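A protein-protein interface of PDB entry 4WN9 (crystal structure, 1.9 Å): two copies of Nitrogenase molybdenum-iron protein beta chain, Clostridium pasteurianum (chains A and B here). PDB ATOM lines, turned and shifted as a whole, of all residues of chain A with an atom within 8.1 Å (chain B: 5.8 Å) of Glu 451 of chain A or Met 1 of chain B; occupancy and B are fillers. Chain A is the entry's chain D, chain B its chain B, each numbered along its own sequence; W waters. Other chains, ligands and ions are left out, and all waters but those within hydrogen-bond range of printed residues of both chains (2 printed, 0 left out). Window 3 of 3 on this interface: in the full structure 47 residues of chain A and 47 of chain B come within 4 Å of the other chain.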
ATOM      1  N   GLU A 446       9.889  -7.950 -24.725  1.00  0.00           N
ATOM      2  CA  GLU A 446       9.234  -7.167 -23.702  1.00  0.00           C
ATOM      3  C   GLU A 446       8.658  -5.885 -24.266  1.00  0.00           C
ATOM      4  O   GLU A 446       7.810  -5.290 -23.663  1.00  0.00           O
ATOM      5  CB  GLU A 446      10.204  -6.890 -22.542  1.00  0.00           C
ATOM      6  CG  GLU A 446      10.864  -8.168 -22.010  1.00  0.00           C
ATOM      7  CD  GLU A 446      11.426  -8.017 -20.616  1.00  0.00           C
ATOM      8  OE1 GLU A 446      12.349  -7.182 -20.438  1.00  0.00           O
ATOM      9  OE2 GLU A 446      10.891  -8.688 -19.696  1.00  0.00           O
ATOM     10  N   ARG A 447       9.131  -5.434 -25.408  1.00  0.00           N
ATOM     11  CA  ARG A 447       8.545  -4.255 -26.022  1.00  0.00           C
ATOM     12  C   ARG A 447       7.189  -4.601 -26.616  1.00  0.00           C
ATOM     13  O   ARG A 447       6.226  -3.849 -26.468  1.00  0.00           O
ATOM     14  CB  ARG A 447       9.443  -3.708 -27.121  1.00  0.00           C
ATOM     15  CG  ARG A 447       9.050  -2.322 -27.552  1.00  0.00           C
ATOM     16  CD  ARG A 447       9.914  -1.804 -28.676  1.00  0.00           C
ATOM     17  NE  ARG A 447      11.318  -1.909 -28.313  1.00  0.00           N
ATOM     18  CZ  ARG A 447      12.144  -2.794 -28.843  1.00  0.00           C
ATOM     19  NH1 ARG A 447      13.411  -2.849 -28.453  1.00  0.00           N
ATOM     20  NH2 ARG A 447      11.694  -3.626 -29.769  1.00  0.00           N
ATOM     21  N   GLU A 448       7.127  -5.763 -27.247  1.00  0.00           N
ATOM     22  CA  GLU A 448       6.011  -6.135 -28.100  1.00  0.00           C
ATOM     23  C   GLU A 448       4.980  -7.026 -27.461  1.00  0.00           C
ATOM     24  O   GLU A 448       3.882  -7.112 -27.968  1.00  0.00           O
ATOM     25  CB  GLU A 448       6.547  -6.819 -29.357  1.00  0.00           C
ATOM     26  CG  GLU A 448       7.394  -5.825 -30.110  1.00  0.00           C
ATOM     27  CD  GLU A 448       7.812  -6.286 -31.461  1.00  0.00           C
ATOM     28  OE1 GLU A 448       7.573  -7.468 -31.771  1.00  0.00           O
ATOM     29  OE2 GLU A 448       8.389  -5.450 -32.190  1.00  0.00           O
ATOM     30  N   CYS A 449       5.328  -7.718 -26.380  1.00  0.00           N
ATOM     31  CA  CYS A 449       4.381  -8.629 -25.757  1.00  0.00           C
ATOM     32  C   CYS A 449       3.141  -7.884 -25.291  1.00  0.00           C
ATOM     33  O   CYS A 449       3.185  -6.689 -24.994  1.00  0.00           O
ATOM     34  CB  CYS A 449       5.025  -9.388 -24.582  1.00  0.00           C
ATOM     35  SG  CYS A 449       5.454  -8.395 -23.131  1.00  0.00           S
ATOM     36  N   THR A 450       2.024  -8.594 -25.204  1.00  0.00           N
ATOM     37  CA  THR A 450       0.862  -8.006 -24.541  1.00  0.00           C
ATOM     38  C   THR A 450       1.216  -7.645 -23.091  1.00  0.00           C
ATOM     39  O   THR A 450       2.109  -8.243 -22.483  1.00  0.00           O
ATOM     40  CB  THR A 450      -0.370  -8.931 -24.563  1.00  0.00           C
ATOM     41  OG1 THR A 450      -0.086 -10.166 -23.886  1.00  0.00           O
ATOM     42  CG2 THR A 450      -0.799  -9.214 -26.009  1.00  0.00           C
ATOM     43  N   GLU A 451       0.523  -6.656 -22.550  1.00  0.00           N
ATOM     44  CA  GLU A 451       0.759  -6.222 -21.195  1.00  0.00           C
ATOM     45  C   GLU A 451       0.557  -7.357 -20.189  1.00  0.00           C
ATOM     46  O   GLU A 451       1.292  -7.458 -19.210  1.00  0.00           O
ATOM     47  CB  GLU A 451      -0.179  -5.084 -20.837  1.00  0.00           C
ATOM     48  CG  GLU A 451       0.040  -3.818 -21.626  1.00  0.00           C
ATOM     49  CD  GLU A 451      -0.465  -2.607 -20.881  1.00  0.00           C
ATOM     50  OE1 GLU A 451      -1.166  -2.773 -19.864  1.00  0.00           O
ATOM     51  OE2 GLU A 451      -0.131  -1.484 -21.284  1.00  0.00           O
ATOM     52  N   GLU A 452      -0.440  -8.205 -20.425  1.00  0.00           N
ATOM     53  CA  GLU A 452      -0.714  -9.311 -19.505  1.00  0.00           C
ATOM     54  C   GLU A 452       0.365 -10.375 -19.642  1.00  0.00           C
ATOM     55  O   GLU A 452       0.539 -11.183 -18.747  1.00  0.00           O
ATOM     56  CB  GLU A 452      -2.111  -9.932 -19.740  1.00  0.00           C
ATOM     57  CG  GLU A 452      -2.245 -10.794 -20.988  1.00  0.00           C
ATOM     58  CD  GLU A 452      -2.853 -10.056 -22.169  1.00  0.00           C
ATOM     59  OE1 GLU A 452      -2.760  -8.811 -22.216  1.00  0.00           O
ATOM     60  OE2 GLU A 452      -3.415 -10.735 -23.061  1.00  0.00           O
ATOM     61  N   ASP A 453       1.088 -10.359 -20.757  1.00  0.00           N
ATOM     62  CA  ASP A 453       2.203 -11.283 -20.954  1.00  0.00           C
ATOM     63  C   ASP A 453       3.531 -10.731 -20.437  1.00  0.00           C
ATOM     64  O   ASP A 453       4.547 -11.402 -20.509  1.00  0.00           O
ATOM     65  CB  ASP A 453       2.347 -11.632 -22.432  1.00  0.00           C
ATOM     66  CG  ASP A 453       1.400 -12.730 -22.866  1.00  0.00           C
ATOM     67  OD1 ASP A 453       0.825 -13.404 -21.997  1.00  0.00           O
ATOM     68  OD2 ASP A 453       1.239 -12.926 -24.084  1.00  0.00           O
ATOM     69  N   PHE A 454       3.513  -9.507 -19.925  1.00  0.00           N
ATOM     70  CA  PHE A 454       4.739  -8.847 -19.440  1.00  0.00           C
ATOM     71  C   PHE A 454       5.225  -9.547 -18.157  1.00  0.00           C
ATOM     72  O   PHE A 454       4.419  -9.998 -17.329  1.00  0.00           O
ATOM     73  CB  PHE A 454       4.457  -7.362 -19.186  1.00  0.00           C
ATOM     74  CG  PHE A 454       5.678  -6.460 -19.229  1.00  0.00           C
ATOM     75  CD1 PHE A 454       6.292  -6.128 -20.443  1.00  0.00           C
ATOM     76  CD2 PHE A 454       6.177  -5.897 -18.055  1.00  0.00           C
ATOM     77  CE1 PHE A 454       7.396  -5.281 -20.484  1.00  0.00           C
ATOM     78  CE2 PHE A 454       7.269  -5.041 -18.093  1.00  0.00           C
ATOM     79  CZ  PHE A 454       7.873  -4.727 -19.316  1.00  0.00           C
ATOM     80  N   GLU A 455       6.542  -9.626 -17.997  1.00  0.00           N
ATOM     81  CA  GLU A 455       7.158 -10.451 -16.979  1.00  0.00           C
ATOM     82  C   GLU A 455       8.083  -9.613 -16.100  1.00  0.00           C
ATOM     83  O   GLU A 455       8.697  -8.669 -16.555  1.00  0.00           O
ATOM     84  CB  GLU A 455       8.005 -11.544 -17.638  1.00  0.00           C
ATOM     85  CG  GLU A 455       7.288 -12.480 -18.614  1.00  0.00           C
ATOM     86  CD  GLU A 455       6.280 -13.385 -17.934  1.00  0.00           C
ATOM     87  OE1 GLU A 455       6.348 -13.503 -16.692  1.00  0.00           O
ATOM     88  OE2 GLU A 455       5.416 -13.967 -18.635  1.00  0.00           O
ATOM     89  N   MET B   1      -0.187   0.370 -19.228  1.00  0.00           N
ATOM     90  CA  MET B   1       0.564  -0.335 -18.148  1.00  0.00           C
ATOM     91  C   MET B   1       0.653   0.581 -16.929  1.00  0.00           C
ATOM     92  O   MET B   1       0.759   1.790 -17.077  1.00  0.00           O
ATOM     93  CB  MET B   1       1.942  -0.758 -18.690  1.00  0.00           C
ATOM     94  CG  MET B   1       2.901  -1.338 -17.648  1.00  0.00           C
ATOM     95  SD  MET B   1       4.288  -2.205 -18.408  1.00  0.00           S
ATOM     96  CE  MET B   1       3.427  -3.621 -19.078  1.00  0.00           C
ATOM     97  N   LEU B   2       0.598   0.019 -15.723  1.00  0.00           N
ATOM     98  CA  LEU B   2       0.505   0.832 -14.506  1.00  0.00           C
ATOM     99  C   LEU B   2      -0.641   1.863 -14.607  1.00  0.00           C
ATOM    100  O   LEU B   2      -0.516   3.029 -14.196  1.00  0.00           O
ATOM    101  CB  LEU B   2       1.834   1.521 -14.209  1.00  0.00           C
ATOM    102  CG  LEU B   2       2.994   0.576 -13.845  1.00  0.00           C
ATOM    103  CD1 LEU B   2       4.328   1.313 -13.939  1.00  0.00           C
ATOM    104  CD2 LEU B   2       2.807  -0.020 -12.456  1.00  0.00           C
ATOM    105  N   ASP B   3      -1.766   1.399 -15.134  1.00  0.00           N
ATOM    106  CA  ASP B   3      -2.915   2.261 -15.400  1.00  0.00           C
ATOM    107  C   ASP B   3      -3.438   2.936 -14.133  1.00  0.00           C
ATOM    108  O   ASP B   3      -3.759   4.114 -14.149  1.00  0.00           O
ATOM    109  CB  ASP B   3      -4.016   1.456 -16.085  1.00  0.00           C
ATOM    110  CG  ASP B   3      -3.611   0.981 -17.446  1.00  0.00           C
ATOM    111  OD1 ASP B   3      -2.541   1.418 -17.921  1.00  0.00           O
ATOM    112  OD2 ASP B   3      -4.343   0.172 -18.052  1.00  0.00           O
ATOM    113  N   HIS B 378       7.214   7.410 -10.817  1.00  0.00           N
ATOM    114  CA  HIS B 378       6.305   7.383 -11.926  1.00  0.00           C
ATOM    115  C   HIS B 378       5.303   8.556 -11.920  1.00  0.00           C
ATOM    116  O   HIS B 378       4.977   9.086 -12.954  1.00  0.00           O
ATOM    117  CB  HIS B 378       5.500   6.094 -11.927  1.00  0.00           C
ATOM    118  CG  HIS B 378       4.749   5.872 -13.196  1.00  0.00           C
ATOM    119  ND1 HIS B 378       3.840   4.852 -13.355  1.00  0.00           N
ATOM    120  CD2 HIS B 378       4.765   6.546 -14.368  1.00  0.00           C
ATOM    121  CE1 HIS B 378       3.323   4.911 -14.566  1.00  0.00           C
ATOM    122  NE2 HIS B 378       3.883   5.916 -15.207  1.00  0.00           N
ATOM    123  N   LYS B 396      11.393  -1.483 -15.307  1.00  0.00           N
ATOM    124  CA  LYS B 396      11.084  -1.849 -16.683  1.00  0.00           C
ATOM    125  C   LYS B 396       9.618  -1.515 -17.015  1.00  0.00           C
ATOM    126  O   LYS B 396       9.264  -1.326 -18.180  1.00  0.00           O
ATOM    127  CB  LYS B 396      11.328  -3.342 -16.898  1.00  0.00           C
ATOM    128  CG  LYS B 396      10.317  -4.182 -16.153  1.00  0.00           C
ATOM    129  CD  LYS B 396      10.642  -5.660 -16.057  1.00  0.00           C
ATOM    130  CE  LYS B 396      10.620  -6.357 -17.378  1.00  0.00           C
ATOM    131  NZ  LYS B 396      11.194  -7.731 -17.251  1.00  0.00           N
ATOM    132  N   PHE B 397       8.773  -1.516 -15.992  1.00  0.00           N
ATOM    133  CA  PHE B 397       7.346  -1.240 -16.148  1.00  0.00           C
ATOM    134  C   PHE B 397       7.104   0.228 -16.513  1.00  0.00           C
ATOM    135  O   PHE B 397       6.270   0.539 -17.338  1.00  0.00           O
ATOM    136  CB  PHE B 397       6.593  -1.534 -14.854  1.00  0.00           C
ATOM    137  CG  PHE B 397       6.463  -3.000 -14.527  1.00  0.00           C
ATOM    138  CD1 PHE B 397       5.430  -3.752 -15.059  1.00  0.00           C
ATOM    139  CD2 PHE B 397       7.344  -3.612 -13.653  1.00  0.00           C
ATOM    140  CE1 PHE B 397       5.298  -5.086 -14.742  1.00  0.00           C
ATOM    141  CE2 PHE B 397       7.206  -4.940 -13.332  1.00  0.00           C
ATOM    142  CZ  PHE B 397       6.188  -5.683 -13.882  1.00  0.00           C
ATOM    143  N   ILE B 398       7.833   1.116 -15.856  1.00  0.00           N
ATOM    144  CA  ILE B 398       7.786   2.540 -16.148  1.00  0.00           C
ATOM    145  C   ILE B 398       8.436   2.824 -17.498  1.00  0.00           C
ATOM    146  O   ILE B 398       7.918   3.610 -18.302  1.00  0.00           O
ATOM    147  CB  ILE B 398       8.510   3.331 -15.050  1.00  0.00           C
ATOM    148  CG1 ILE B 398       7.810   3.120 -13.710  1.00  0.00           C
ATOM    149  CG2 ILE B 398       8.573   4.822 -15.390  1.00  0.00           C
ATOM    150  CD1 ILE B 398       8.492   3.847 -12.584  1.00  0.00           C
ATOM    151  N   ARG B 400       8.538   0.993 -20.031  1.00  0.00           N
ATOM    152  CA  ARG B 400       7.618   0.624 -21.102  1.00  0.00           C
ATOM    153  C   ARG B 400       6.417   1.566 -21.167  1.00  0.00           C
ATOM    154  O   ARG B 400       6.038   2.026 -22.253  1.00  0.00           O
ATOM    155  CB  ARG B 400       7.100  -0.802 -20.935  1.00  0.00           C
ATOM    156  CG  ARG B 400       5.851  -1.052 -21.771  1.00  0.00           C
ATOM    157  CD  ARG B 400       5.782  -2.466 -22.316  1.00  0.00           C
ATOM    158  NE  ARG B 400       4.491  -2.707 -22.927  1.00  0.00           N
ATOM    159  CZ  ARG B 400       4.136  -3.839 -23.518  1.00  0.00           C
ATOM    160  NH1 ARG B 400       4.995  -4.840 -23.626  1.00  0.00           N
ATOM    161  NH2 ARG B 400       2.917  -3.958 -24.018  1.00  0.00           N
ATOM    162  N   GLU B 401       5.798   1.812 -20.017  1.00  0.00           N
ATOM    163  CA  GLU B 401       4.610   2.660 -19.961  1.00  0.00           C
ATOM    164  C   GLU B 401       4.902   4.053 -20.526  1.00  0.00           C
ATOM    165  O   GLU B 401       4.127   4.557 -21.314  1.00  0.00           O
ATOM    166  CB  GLU B 401       4.056   2.728 -18.536  1.00  0.00           C
ATOM    167  CG  GLU B 401       2.950   3.751 -18.306  1.00  0.00           C
ATOM    168  CD  GLU B 401       1.698   3.507 -19.136  1.00  0.00           C
ATOM    169  OE1 GLU B 401       1.565   2.448 -19.786  1.00  0.00           O
ATOM    170  OE2 GLU B 401       0.830   4.394 -19.126  1.00  0.00           O
HETATM  171  O   HOH W   1      -3.761  -2.201 -19.135  1.00  0.00           O
HETATM  172  O   HOH W   2       2.072  -1.174 -22.512  1.00  0.00           O
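OE2 of Glu 451 of chain A lies within hydrogen-bond range of N of Met 1 of chain B.
NH1 of Arg 400 of chain B is in hydrogen-bond range of O of Arg 447 of chain A (3.3 Å).
The backbone carbonyl oxygen (O) of Glu 446 of chain A sits at hydrogen-bond distance from the guanidinium group (NH1) of Arg 400 of chain B (2.9 Å).
The guanidinium group (NH2) of Arg 400 of chain B is in hydrogen-bond range of the backbone carbonyl oxygen (O) of Cys 449 of chain A, at 2.9 Å.
The side-chain amino group (NZ) of Lys 396 of chain B is in salt-bridge range of the side-chain carboxylate (OE2) of Glu 446 of chain A.
The backbone carbonyl oxygen (O) of Glu 455 of chain A sits at hydrogen-bond distance from the side-chain amino group (NZ) of Lys 396 of chain B, 2.8 Å away.
OD1 of Asp 3 of chain B is in hydrogen-bond range of N of Met 1 of chain B, 2.9 Å away.
N of Met 1 of chain B lies within hydrogen-bond range of OE1 of Glu 401 of chain B (2.8 Å).
Arg 400 of chain B touches Glu 451 of chain A.
CG of Phe 454 of chain A touches CE of Met 1 of chain B (3.6 Å).
CE2 of Phe 454 of chain A touches CE of Lys 396 of chain B, at 3.7 Å.
Phe 454 of chain A touches Phe 397 of chain B.
Arg 400 of chain B touches Phe 454 of chain A.
Glu 451 of chain A touches two residues of chain B.
Of the printed residues of chain B, Phe 454 of chain A touches Met 1 (3.6 Å), Lys 396 (3.7 Å), Phe 397 (3.5 Å) and Arg 400 (3.7 Å).
Printed residues of chain B within 4 Å of Glu 455 of chain A: Lys 396 (2.8 Å).
Met 1 of chain B touches just these residues of chain A: Glu 451 and Phe 454.
The nearest printed residue of chain A that does not touch Arg 400 of chain B is Thr 450 of chain A (4.2 Å).
Of the 10 printed residues of chain A, 6 touch a printed residue of chain B.
Of the 9 printed residues of chain B, 4 touch a printed residue of chain A.
Printed residues of chain B that touch a printed residue of chain A: Met 1, Lys 396, Phe 397 and Arg 400.
Among the printed residues, Asp or Glu carboxylates within 4 Å of a Lys or Arg side-chain nitrogen of the other chain: Glu 446 of chain A with Lys 396 of chain B.
No position is printed for both chains.
Of the 11 pairs that touch across the chains among the printed residues, none has its exchanged pair printed and touching as well.
Water W2 bridges the side-chain carboxylate (OE2) of Glu 451 of chain A (2.5 Å) and the guanidinium group (NE) of Arg 400 of chain B (2.9 Å).
Water W1 lies within hydrogen-bond range of the side-chain carboxylate of Asp 3 of chain B and the side-chain carboxylate of Glu 451 of chain A.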
